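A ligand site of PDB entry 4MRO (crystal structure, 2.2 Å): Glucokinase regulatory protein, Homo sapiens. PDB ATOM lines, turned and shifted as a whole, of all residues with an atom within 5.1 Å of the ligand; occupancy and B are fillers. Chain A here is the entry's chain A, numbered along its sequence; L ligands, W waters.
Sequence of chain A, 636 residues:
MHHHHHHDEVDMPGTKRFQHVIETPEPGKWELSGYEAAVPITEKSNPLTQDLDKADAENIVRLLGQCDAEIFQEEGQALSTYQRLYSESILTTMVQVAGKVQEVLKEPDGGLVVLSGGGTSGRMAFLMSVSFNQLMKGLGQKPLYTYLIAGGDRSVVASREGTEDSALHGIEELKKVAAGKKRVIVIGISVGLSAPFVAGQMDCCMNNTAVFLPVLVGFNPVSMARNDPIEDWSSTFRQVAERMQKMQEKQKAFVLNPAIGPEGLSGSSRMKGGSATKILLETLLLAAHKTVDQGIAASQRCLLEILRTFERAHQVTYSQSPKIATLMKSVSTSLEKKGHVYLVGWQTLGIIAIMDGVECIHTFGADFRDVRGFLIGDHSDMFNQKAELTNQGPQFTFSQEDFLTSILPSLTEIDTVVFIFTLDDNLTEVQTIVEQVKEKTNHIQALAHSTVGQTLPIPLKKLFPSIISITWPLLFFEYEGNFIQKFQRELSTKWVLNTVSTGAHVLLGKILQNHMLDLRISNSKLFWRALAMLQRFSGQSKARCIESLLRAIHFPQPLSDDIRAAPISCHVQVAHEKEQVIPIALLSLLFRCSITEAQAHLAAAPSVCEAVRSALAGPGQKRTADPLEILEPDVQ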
ATOM      1  N   HIS A  20      21.785  17.130  19.211  1.00  0.00           N
ATOM      2  CA  HIS A  20      22.885  17.163  18.262  1.00  0.00           C
ATOM      3  C   HIS A  20      22.623  18.031  16.984  1.00  0.00           C
ATOM      4  O   HIS A  20      23.556  18.358  16.228  1.00  0.00           O
ATOM      5  CB  HIS A  20      23.204  15.734  17.864  1.00  0.00           C
ATOM      6  CG  HIS A  20      22.065  15.019  17.211  1.00  0.00           C
ATOM      7  ND1 HIS A  20      22.002  14.805  15.837  1.00  0.00           N
ATOM      8  CD2 HIS A  20      20.930  14.490  17.740  1.00  0.00           C
ATOM      9  CE1 HIS A  20      20.889  14.146  15.554  1.00  0.00           C
ATOM     10  NE2 HIS A  20      20.215  13.953  16.690  1.00  0.00           N
ATOM     11  N   TYR A  35      28.135  25.794  10.915  1.00  0.00           N
ATOM     12  CA  TYR A  35      27.298  24.623  10.699  1.00  0.00           C
ATOM     13  C   TYR A  35      28.010  23.735   9.686  1.00  0.00           C
ATOM     14  O   TYR A  35      27.960  22.536   9.823  1.00  0.00           O
ATOM     15  CB  TYR A  35      25.956  25.042  10.148  1.00  0.00           C
ATOM     16  CG  TYR A  35      25.057  23.943   9.710  1.00  0.00           C
ATOM     17  CD1 TYR A  35      25.263  23.298   8.516  1.00  0.00           C
ATOM     18  CD2 TYR A  35      23.988  23.574  10.451  1.00  0.00           C
ATOM     19  CE1 TYR A  35      24.428  22.303   8.093  1.00  0.00           C
ATOM     20  CE2 TYR A  35      23.139  22.552  10.039  1.00  0.00           C
ATOM     21  CZ  TYR A  35      23.376  21.934   8.865  1.00  0.00           C
ATOM     22  OH  TYR A  35      22.583  20.942   8.445  1.00  0.00           O
ATOM     23  N   VAL A  39      29.557  19.445   9.159  1.00  0.00           N
ATOM     24  CA  VAL A  39      28.982  18.424   8.275  1.00  0.00           C
ATOM     25  C   VAL A  39      30.091  17.461   7.942  1.00  0.00           C
ATOM     26  O   VAL A  39      31.122  17.869   7.357  1.00  0.00           O
ATOM     27  CB  VAL A  39      28.364  18.989   6.979  1.00  0.00           C
ATOM     28  CG1 VAL A  39      27.825  17.850   6.077  1.00  0.00           C
ATOM     29  CG2 VAL A  39      27.251  19.993   7.307  1.00  0.00           C
ATOM     30  N   PRO A  40      29.908  16.190   8.318  1.00  0.00           N
ATOM     31  CA  PRO A  40      30.949  15.188   8.004  1.00  0.00           C
ATOM     32  C   PRO A  40      31.303  15.209   6.538  1.00  0.00           C
ATOM     33  O   PRO A  40      30.440  15.472   5.705  1.00  0.00           O
ATOM     34  CB  PRO A  40      30.284  13.866   8.369  1.00  0.00           C
ATOM     35  CG  PRO A  40      29.121  14.213   9.258  1.00  0.00           C
ATOM     36  CD  PRO A  40      28.669  15.554   8.829  1.00  0.00           C
ATOM     37  N   THR A  42      31.580  12.924   4.524  1.00  0.00           N
ATOM     38  CA  THR A  42      30.852  11.955   3.744  1.00  0.00           C
ATOM     39  C   THR A  42      29.463  12.435   3.366  1.00  0.00           C
ATOM     40  O   THR A  42      28.864  11.919   2.412  1.00  0.00           O
ATOM     41  CB  THR A  42      30.738  10.613   4.494  1.00  0.00           C
ATOM     42  OG1 THR A  42      30.120  10.770   5.794  1.00  0.00           O
ATOM     43  CG2 THR A  42      32.109  10.029   4.680  1.00  0.00           C
ATOM     44  N   GLU A  43      28.940  13.414   4.092  1.00  0.00           N
ATOM     45  CA  GLU A  43      27.600  13.946   3.813  1.00  0.00           C
ATOM     46  C   GLU A  43      27.615  15.220   3.042  1.00  0.00           C
ATOM     47  O   GLU A  43      26.573  15.695   2.619  1.00  0.00           O
ATOM     48  CB  GLU A  43      26.859  14.185   5.146  1.00  0.00           C
ATOM     49  CG  GLU A  43      26.779  12.892   5.935  1.00  0.00           C
ATOM     50  CD  GLU A  43      25.746  11.927   5.404  1.00  0.00           C
ATOM     51  OE1 GLU A  43      24.801  12.346   4.711  1.00  0.00           O
ATOM     52  OE2 GLU A  43      25.888  10.730   5.666  1.00  0.00           O
ATOM     53  N   LYS A  44      28.794  15.792   2.885  1.00  0.00           N
ATOM     54  CA  LYS A  44      28.890  17.098   2.278  1.00  0.00           C
ATOM     55  C   LYS A  44      28.379  17.107   0.830  1.00  0.00           C
ATOM     56  O   LYS A  44      28.265  16.057   0.193  1.00  0.00           O
ATOM     57  CB  LYS A  44      30.339  17.639   2.355  1.00  0.00           C
ATOM     58  CG  LYS A  44      30.756  18.313   3.673  1.00  0.00           C
ATOM     59  CD  LYS A  44      32.170  18.902   3.522  1.00  0.00           C
ATOM     60  CE  LYS A  44      32.961  19.040   4.796  1.00  0.00           C
ATOM     61  NZ  LYS A  44      32.203  19.871   5.771  1.00  0.00           N
ATOM     62  N   SER A  45      28.086  18.329   0.363  1.00  0.00           N
ATOM     63  CA  SER A  45      27.814  18.632  -1.025  1.00  0.00           C
ATOM     64  C   SER A  45      29.138  18.791  -1.767  1.00  0.00           C
ATOM     65  O   SER A  45      29.955  19.632  -1.402  1.00  0.00           O
ATOM     66  CB  SER A  45      27.071  19.982  -1.124  1.00  0.00           C
ATOM     67  OG  SER A  45      26.896  20.344  -2.479  1.00  0.00           O
ATOM     68  N   GLY A 192      30.790   6.368   6.764  1.00  0.00           N
ATOM     69  CA  GLY A 192      30.507   7.546   7.510  1.00  0.00           C
ATOM     70  C   GLY A 192      30.993   7.477   8.922  1.00  0.00           C
ATOM     71  O   GLY A 192      30.845   8.450   9.636  1.00  0.00           O
ATOM     72  N   LEU A 193      31.602   6.375   9.330  1.00  0.00           N
ATOM     73  CA  LEU A 193      31.891   6.143  10.753  1.00  0.00           C
ATOM     74  C   LEU A 193      30.559   6.386  11.548  1.00  0.00           C
ATOM     75  O   LEU A 193      30.450   7.151  12.527  1.00  0.00           O
ATOM     76  CB  LEU A 193      32.978   7.084  11.219  1.00  0.00           C
ATOM     77  CG  LEU A 193      34.398   6.959  10.651  1.00  0.00           C
ATOM     78  CD1 LEU A 193      35.378   7.755  11.516  1.00  0.00           C
ATOM     79  CD2 LEU A 193      34.822   5.516  10.655  1.00  0.00           C
ATOM     80  N   SER A 194      29.550   5.695  11.064  1.00  0.00           N
ATOM     81  CA  SER A 194      28.178   5.983  11.339  1.00  0.00           C
ATOM     82  C   SER A 194      27.403   4.772  11.867  1.00  0.00           C
ATOM     83  O   SER A 194      26.544   4.995  12.669  1.00  0.00           O
ATOM     84  CB  SER A 194      27.512   6.434  10.060  1.00  0.00           C
ATOM     85  OG  SER A 194      26.094   6.205  10.137  1.00  0.00           O
ATOM     86  N   ASN A 220      35.855   9.460   7.416  1.00  0.00           N
ATOM     87  CA  ASN A 220      35.738  10.759   8.083  1.00  0.00           C
ATOM     88  C   ASN A 220      36.836  10.854   9.132  1.00  0.00           C
ATOM     89  O   ASN A 220      37.256   9.863   9.688  1.00  0.00           O
ATOM     90  CB  ASN A 220      34.356  10.928   8.751  1.00  0.00           C
ATOM     91  CG  ASN A 220      33.264  11.369   7.803  1.00  0.00           C
ATOM     92  OD1 ASN A 220      33.414  12.307   7.023  1.00  0.00           O
ATOM     93  ND2 ASN A 220      32.146  10.667   7.856  1.00  0.00           N
ATOM     94  N   MET A 224      34.680  13.869  13.195  1.00  0.00           N
ATOM     95  CA  MET A 224      33.401  14.026  12.542  1.00  0.00           C
ATOM     96  C   MET A 224      32.626  12.735  12.584  1.00  0.00           C
ATOM     97  O   MET A 224      31.646  12.576  11.822  1.00  0.00           O
ATOM     98  CB  MET A 224      33.621  14.391  11.075  1.00  0.00           C
ATOM     99  CG  MET A 224      33.909  15.838  10.811  1.00  0.00           C
ATOM    100  SD  MET A 224      34.578  15.888   9.155  1.00  0.00           S
ATOM    101  CE  MET A 224      34.711  17.673   8.899  1.00  0.00           C
ATOM    102  N   ALA A 225      33.047  11.775  13.399  1.00  0.00           N
ATOM    103  CA  ALA A 225      32.330  10.513  13.523  1.00  0.00           C
ATOM    104  C   ALA A 225      30.976  10.774  14.134  1.00  0.00           C
ATOM    105  O   ALA A 225      30.825  11.693  14.924  1.00  0.00           O
ATOM    106  CB  ALA A 225      33.072   9.561  14.401  1.00  0.00           C
ATOM    107  N   ARG A 226      30.009   9.956  13.776  1.00  0.00           N
ATOM    108  CA  ARG A 226      28.645  10.137  14.252  1.00  0.00           C
ATOM    109  C   ARG A 226      28.553  10.132  15.776  1.00  0.00           C
ATOM    110  O   ARG A 226      29.244   9.355  16.463  1.00  0.00           O
ATOM    111  CB  ARG A 226      27.791   9.040  13.666  1.00  0.00           C
ATOM    112  CG  ARG A 226      26.358   9.303  13.787  1.00  0.00           C
ATOM    113  CD  ARG A 226      25.597   8.378  12.870  1.00  0.00           C
ATOM    114  NE  ARG A 226      24.232   8.430  13.258  1.00  0.00           N
ATOM    115  CZ  ARG A 226      23.250   7.657  12.803  1.00  0.00           C
ATOM    116  NH1 ARG A 226      23.463   6.739  11.887  1.00  0.00           N
ATOM    117  NH2 ARG A 226      22.023   7.831  13.321  1.00  0.00           N
ATOM    118  N   ASN A 227      27.701  11.010  16.277  1.00  0.00           N
ATOM    119  CA  ASN A 227      27.636  11.288  17.706  1.00  0.00           C
ATOM    120  C   ASN A 227      26.251  11.449  18.274  1.00  0.00           C
ATOM    121  O   ASN A 227      26.166  11.874  19.356  1.00  0.00           O
ATOM    122  CB  ASN A 227      28.501  12.539  18.077  1.00  0.00           C
ATOM    123  CG  ASN A 227      28.981  12.536  19.543  1.00  0.00           C
ATOM    124  OD1 ASN A 227      29.452  11.547  20.092  1.00  0.00           O
ATOM    125  ND2 ASN A 227      28.864  13.670  20.175  1.00  0.00           N
ATOM    126  N   ASP A 228      25.185  11.085  17.584  1.00  0.00           N
ATOM    127  CA  ASP A 228      23.857  11.028  18.186  1.00  0.00           C
ATOM    128  C   ASP A 228      23.695   9.645  18.846  1.00  0.00           C
ATOM    129  O   ASP A 228      24.329   8.716  18.434  1.00  0.00           O
ATOM    130  CB  ASP A 228      22.737  11.282  17.143  1.00  0.00           C
ATOM    131  CG  ASP A 228      22.823  10.359  15.936  1.00  0.00           C
ATOM    132  OD1 ASP A 228      23.904  10.262  15.350  1.00  0.00           O
ATOM    133  OD2 ASP A 228      21.836   9.733  15.538  1.00  0.00           O
ATOM    134  N   SER A 266      25.615  13.565  -3.005  1.00  0.00           N
ATOM    135  CA  SER A 266      25.755  13.770  -1.593  1.00  0.00           C
ATOM    136  C   SER A 266      25.275  12.599  -0.786  1.00  0.00           C
ATOM    137  O   SER A 266      24.116  12.214  -0.906  1.00  0.00           O
ATOM    138  CB  SER A 266      25.001  15.025  -1.141  1.00  0.00           C
ATOM    139  OG  SER A 266      25.249  16.082  -2.036  1.00  0.00           O
ATOM    140  N   HIS A 515      21.697  16.460  -4.629  1.00  0.00           N
ATOM    141  CA  HIS A 515      21.003  15.833  -3.505  1.00  0.00           C
ATOM    142  C   HIS A 515      19.816  15.004  -4.030  1.00  0.00           C
ATOM    143  O   HIS A 515      19.106  15.429  -4.967  1.00  0.00           O
ATOM    144  CB  HIS A 515      20.464  16.904  -2.556  1.00  0.00           C
ATOM    145  CG  HIS A 515      21.528  17.815  -1.998  1.00  0.00           C
ATOM    146  ND1 HIS A 515      22.526  17.359  -1.167  1.00  0.00           N
ATOM    147  CD2 HIS A 515      21.751  19.137  -2.174  1.00  0.00           C
ATOM    148  CE1 HIS A 515      23.309  18.364  -0.839  1.00  0.00           C
ATOM    149  NE2 HIS A 515      22.855  19.449  -1.426  1.00  0.00           N
ATOM    150  N   SER A 524      17.877   5.694  10.765  1.00  0.00           N
ATOM    151  CA  SER A 524      18.102   6.937  11.492  1.00  0.00           C
ATOM    152  C   SER A 524      18.983   7.925  10.661  1.00  0.00           C
ATOM    153  O   SER A 524      18.717   9.133  10.560  1.00  0.00           O
ATOM    154  CB  SER A 524      18.770   6.590  12.802  1.00  0.00           C
ATOM    155  OG  SER A 524      20.012   5.920  12.583  1.00  0.00           O
ATOM    156  N   LYS A 525      20.027   7.394  10.032  1.00  0.00           N
ATOM    157  CA  LYS A 525      20.898   8.254   9.231  1.00  0.00           C
ATOM    158  C   LYS A 525      20.142   9.015   8.098  1.00  0.00           C
ATOM    159  O   LYS A 525      20.311  10.231   7.897  1.00  0.00           O
ATOM    160  CB  LYS A 525      22.098   7.454   8.699  1.00  0.00           C
ATOM    161  CG  LYS A 525      22.973   8.239   7.734  1.00  0.00           C
ATOM    162  CD  LYS A 525      24.206   7.418   7.247  1.00  0.00           C
ATOM    163  CE  LYS A 525      23.839   6.345   6.231  1.00  0.00           C
ATOM    164  NZ  LYS A 525      24.941   5.388   6.210  1.00  0.00           N
ATOM    165  N   TRP A 528      18.188  11.787   9.550  1.00  0.00           N
ATOM    166  CA  TRP A 528      18.966  13.037   9.754  1.00  0.00           C
ATOM    167  C   TRP A 528      19.265  13.697   8.436  1.00  0.00           C
ATOM    168  O   TRP A 528      19.306  14.932   8.355  1.00  0.00           O
ATOM    169  CB  TRP A 528      20.263  12.808  10.556  1.00  0.00           C
ATOM    170  CG  TRP A 528      19.956  12.169  11.871  1.00  0.00           C
ATOM    171  CD1 TRP A 528      20.395  10.964  12.317  1.00  0.00           C
ATOM    172  CD2 TRP A 528      19.120  12.692  12.899  1.00  0.00           C
ATOM    173  NE1 TRP A 528      19.906  10.712  13.563  1.00  0.00           N
ATOM    174  CE2 TRP A 528      19.119  11.753  13.942  1.00  0.00           C
ATOM    175  CE3 TRP A 528      18.413  13.874  13.049  1.00  0.00           C
ATOM    176  CZ2 TRP A 528      18.405  11.944  15.110  1.00  0.00           C
ATOM    177  CZ3 TRP A 528      17.689  14.079  14.236  1.00  0.00           C
ATOM    178  CH2 TRP A 528      17.676  13.097  15.232  1.00  0.00           C
ATOM    179  N   ARG A 529      19.478  12.899   7.378  1.00  0.00           N
ATOM    180  CA  ARG A 529      19.765  13.480   6.066  1.00  0.00           C
ATOM    181  C   ARG A 529      18.528  14.254   5.591  1.00  0.00           C
ATOM    182  O   ARG A 529      18.630  15.385   5.091  1.00  0.00           O
ATOM    183  CB  ARG A 529      20.217  12.445   5.017  1.00  0.00           C
ATOM    184  CG  ARG A 529      20.734  13.061   3.690  1.00  0.00           C
ATOM    185  CD  ARG A 529      21.569  12.079   2.865  1.00  0.00           C
ATOM    186  NE  ARG A 529      22.586  11.279   3.619  1.00  0.00           N
ATOM    187  CZ  ARG A 529      22.863   9.963   3.418  1.00  0.00           C
ATOM    188  NH1 ARG A 529      22.171   9.264   2.536  1.00  0.00           N
ATOM    189  NH2 ARG A 529      23.806   9.322   4.121  1.00  0.00           N
ATOM    190  N   ALA A 532      18.319  17.522   7.600  1.00  0.00           N
ATOM    191  CA  ALA A 532      19.317  18.400   6.999  1.00  0.00           C
ATOM    192  C   ALA A 532      18.915  19.031   5.662  1.00  0.00           C
ATOM    193  O   ALA A 532      19.187  20.215   5.391  1.00  0.00           O
ATOM    194  CB  ALA A 532      20.605  17.633   6.792  1.00  0.00           C
ATOM    195  N   MET A 533      18.331  18.234   4.776  1.00  0.00           N
ATOM    196  CA  MET A 533      17.923  18.777   3.477  1.00  0.00           C
ATOM    197  C   MET A 533      16.772  19.774   3.652  1.00  0.00           C
ATOM    198  O   MET A 533      16.734  20.811   2.990  1.00  0.00           O
ATOM    199  CB  MET A 533      17.571  17.648   2.548  1.00  0.00           C
ATOM    200  CG  MET A 533      18.810  16.937   2.061  1.00  0.00           C
ATOM    201  SD  MET A 533      18.425  15.700   0.858  1.00  0.00           S
ATOM    202  CE  MET A 533      17.363  14.622   1.745  1.00  0.00           C
ATOM    203  N   ARG A 536      18.429  23.068   4.659  1.00  0.00           N
ATOM    204  CA  ARG A 536      19.242  23.664   3.626  1.00  0.00           C
ATOM    205  C   ARG A 536      18.367  24.347   2.562  1.00  0.00           C
ATOM    206  O   ARG A 536      18.599  25.481   2.213  1.00  0.00           O
ATOM    207  CB  ARG A 536      20.153  22.602   2.956  1.00  0.00           C
ATOM    208  CG  ARG A 536      20.985  23.080   1.755  1.00  0.00           C
ATOM    209  CD  ARG A 536      22.167  23.941   2.156  1.00  0.00           C
ATOM    210  NE  ARG A 536      23.213  23.173   2.858  1.00  0.00           N
ATOM    211  CZ  ARG A 536      24.449  23.620   3.129  1.00  0.00           C
ATOM    212  NH1 ARG A 536      24.806  24.846   2.771  1.00  0.00           N
ATOM    213  NH2 ARG A 536      25.329  22.850   3.759  1.00  0.00           N
HETATM  214  C1  LIG L   1      26.085  10.711   9.901  1.00  0.00           C
HETATM  215  C2  LIG L   1      27.426  10.463   9.802  1.00  0.00           C
HETATM  216  C3  LIG L   1      28.297  11.123  10.661  1.00  0.00           C
HETATM  217  N1  LIG L   1      29.589  10.883  10.567  1.00  0.00           N
HETATM  218  N2  LIG L   1      27.837  12.017  11.572  1.00  0.00           N
HETATM  219  C4  LIG L   1      26.530  12.289  11.661  1.00  0.00           C
HETATM  220  C5  LIG L   1      25.616  11.628  10.839  1.00  0.00           C
HETATM  221  S1  LIG L   1      23.921  12.006  10.890  1.00  0.00           S
HETATM  222  O1  LIG L   1      23.144  10.793  10.512  1.00  0.00           O
HETATM  223  O2  LIG L   1      23.577  12.590  12.190  1.00  0.00           O
HETATM  224  N3  LIG L   1      23.612  13.184   9.842  1.00  0.00           N
HETATM  225  C6  LIG L   1      23.787  12.734   8.497  1.00  0.00           C
HETATM  226  C7  LIG L   1      23.335  13.841   7.566  1.00  0.00           C
HETATM  227  C8  LIG L   1      24.583  14.257  10.097  1.00  0.00           C
HETATM  228  C9  LIG L   1      24.393  15.488   9.163  1.00  0.00           C
HETATM  229  N4  LIG L   1      23.964  15.137   7.815  1.00  0.00           N
HETATM  230  C10 LIG L   1      23.874  16.104   6.813  1.00  0.00           C
HETATM  231  C11 LIG L   1      23.534  15.753   5.491  1.00  0.00           C
HETATM  232  C12 LIG L   1      23.452  16.684   4.452  1.00  0.00           C
HETATM  233  C13 LIG L   1      24.098  17.409   7.061  1.00  0.00           C
HETATM  234  C14 LIG L   1      23.999  18.376   6.048  1.00  0.00           C
HETATM  235  C15 LIG L   1      23.670  18.033   4.726  1.00  0.00           C
HETATM  236  C16 LIG L   1      23.540  19.113   3.670  1.00  0.00           C
HETATM  237  C17 LIG L   1      22.241  18.990   2.901  1.00  0.00           C
HETATM  238  F1  LIG L   1      22.100  20.071   2.085  1.00  0.00           F
HETATM  239  F2  LIG L   1      21.258  18.895   3.793  1.00  0.00           F
HETATM  240  F3  LIG L   1      22.271  17.892   2.169  1.00  0.00           F
HETATM  241  C18 LIG L   1      24.718  19.136   2.748  1.00  0.00           C
HETATM  242  F4  LIG L   1      25.799  19.351   3.493  1.00  0.00           F
HETATM  243  F5  LIG L   1      24.736  17.971   2.041  1.00  0.00           F
HETATM  244  F6  LIG L   1      24.634  20.177   1.921  1.00  0.00           F
HETATM  245  O3  LIG L   1      23.393  20.334   4.322  1.00  0.00           O
HETATM  246  O   HOH W   1      21.607  21.014   5.919  1.00  0.00           O
HETATM  247  O   HOH W   2      28.829  13.953  12.997  1.00  0.00           O
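O of Gly 192 sits at hydrogen-bond distance from N1 of the ligand (2.9 Å). O of Met 224 is in hydrogen-bond range of N1 of the ligand (2.9 Å). NE of Arg 536 is in hydrogen-bond range of O3 of the ligand (3.2 Å).
A ring nitrogen (ND1) of His 515 lies within hydrogen-bond range of the side-chain hydroxyl of Ser 266 (3.1 Å). OD2 of Asp 228 lies within hydrogen-bond range of NE1 of Trp 528. The guanidinium group (NE) of Arg 226 lies within salt-bridge range of the side-chain carboxylate (OD1) of Asp 228, 2.8 Å away. The guanidinium group (NH1) of Arg 226 is in hydrogen-bond range of the side-chain hydroxyl (OG) of Ser 194 (3.2 Å). The backbone carbonyl oxygen (O) of Leu 193 lies within hydrogen-bond range of the backbone NH (N) of Arg 226, 3.1 Å away. NH2 of Arg 226 is in hydrogen-bond range of OG of Ser 524, 2.9 Å away. O of Val 39 is in hydrogen-bond range of NZ of Lys 44 (2.8 Å). The side-chain amide nitrogen (ND2) of Asn 220 is in hydrogen-bond range of the side-chain hydroxyl (OG1) of Thr 42 (2.9 Å).
A fluorine (F5) of the ligand lies close to the backbone carbonyl oxygen (O) of Glu 43, at 3.0 Å. A nitrogen (N1) of the ligand sits close to the backbone NH (N) of Arg 226 (3.4 Å). ND1 of His 515 sits close to F3 of the ligand (3.4 Å). F2 of the ligand sits close to O of Ala 532 (2.9 Å). N of Met 533 lies close to F2 of the ligand, 3.2 Å away. Tyr 35 touches the ligand. Val 39 touches the ligand (CG1 to F4, 3.6 Å). Pro 40 touches the ligand (CG to N2, 3.4 Å). Lys 44 touches the ligand. Ser 45 touches the ligand (N to F5, 3.8 Å). Asn 220 touches the ligand (ND2 to N1, 3.7 Å). C of Ala 225 touches N1 of the ligand (3.8 Å). Asp 228 touches the ligand (OD1 to O2, 3.9 Å). Lys 525 touches the ligand (CA to O1, 3.6 Å). Trp 528 touches the ligand (CD1 to O1, 3.3 Å). Arg 529 touches the ligand (CA to C7, 3.9 Å). Hydrophobic or aromatic side chains that line the ligand: Val 39, Pro 40, His 515, Trp 528, Ala 532 and Met 533. Within 4 Å of the ligand: Tyr 35, Val 39, Pro 40, Glu 43, Lys 44, Ser 45, Gly 192, Asn 220, Met 224, Ala 225, Arg 226, Asp 228, His 515, Lys 525, Trp 528, Arg 529, Ala 532, Met 533 and Arg 536.
Water W1 lies within hydrogen-bond range of an oxygen (O3) of the ligand (2.5 Å), the backbone carbonyl oxygen of Ala 532 (2.6 Å) and the side-chain hydroxyl of Tyr 35 (2.7 Å). Water W2 bridges a nitrogen (N2) of the ligand (2.6 Å) and the backbone carbonyl oxygen (O) of Met 224 (3.3 Å).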
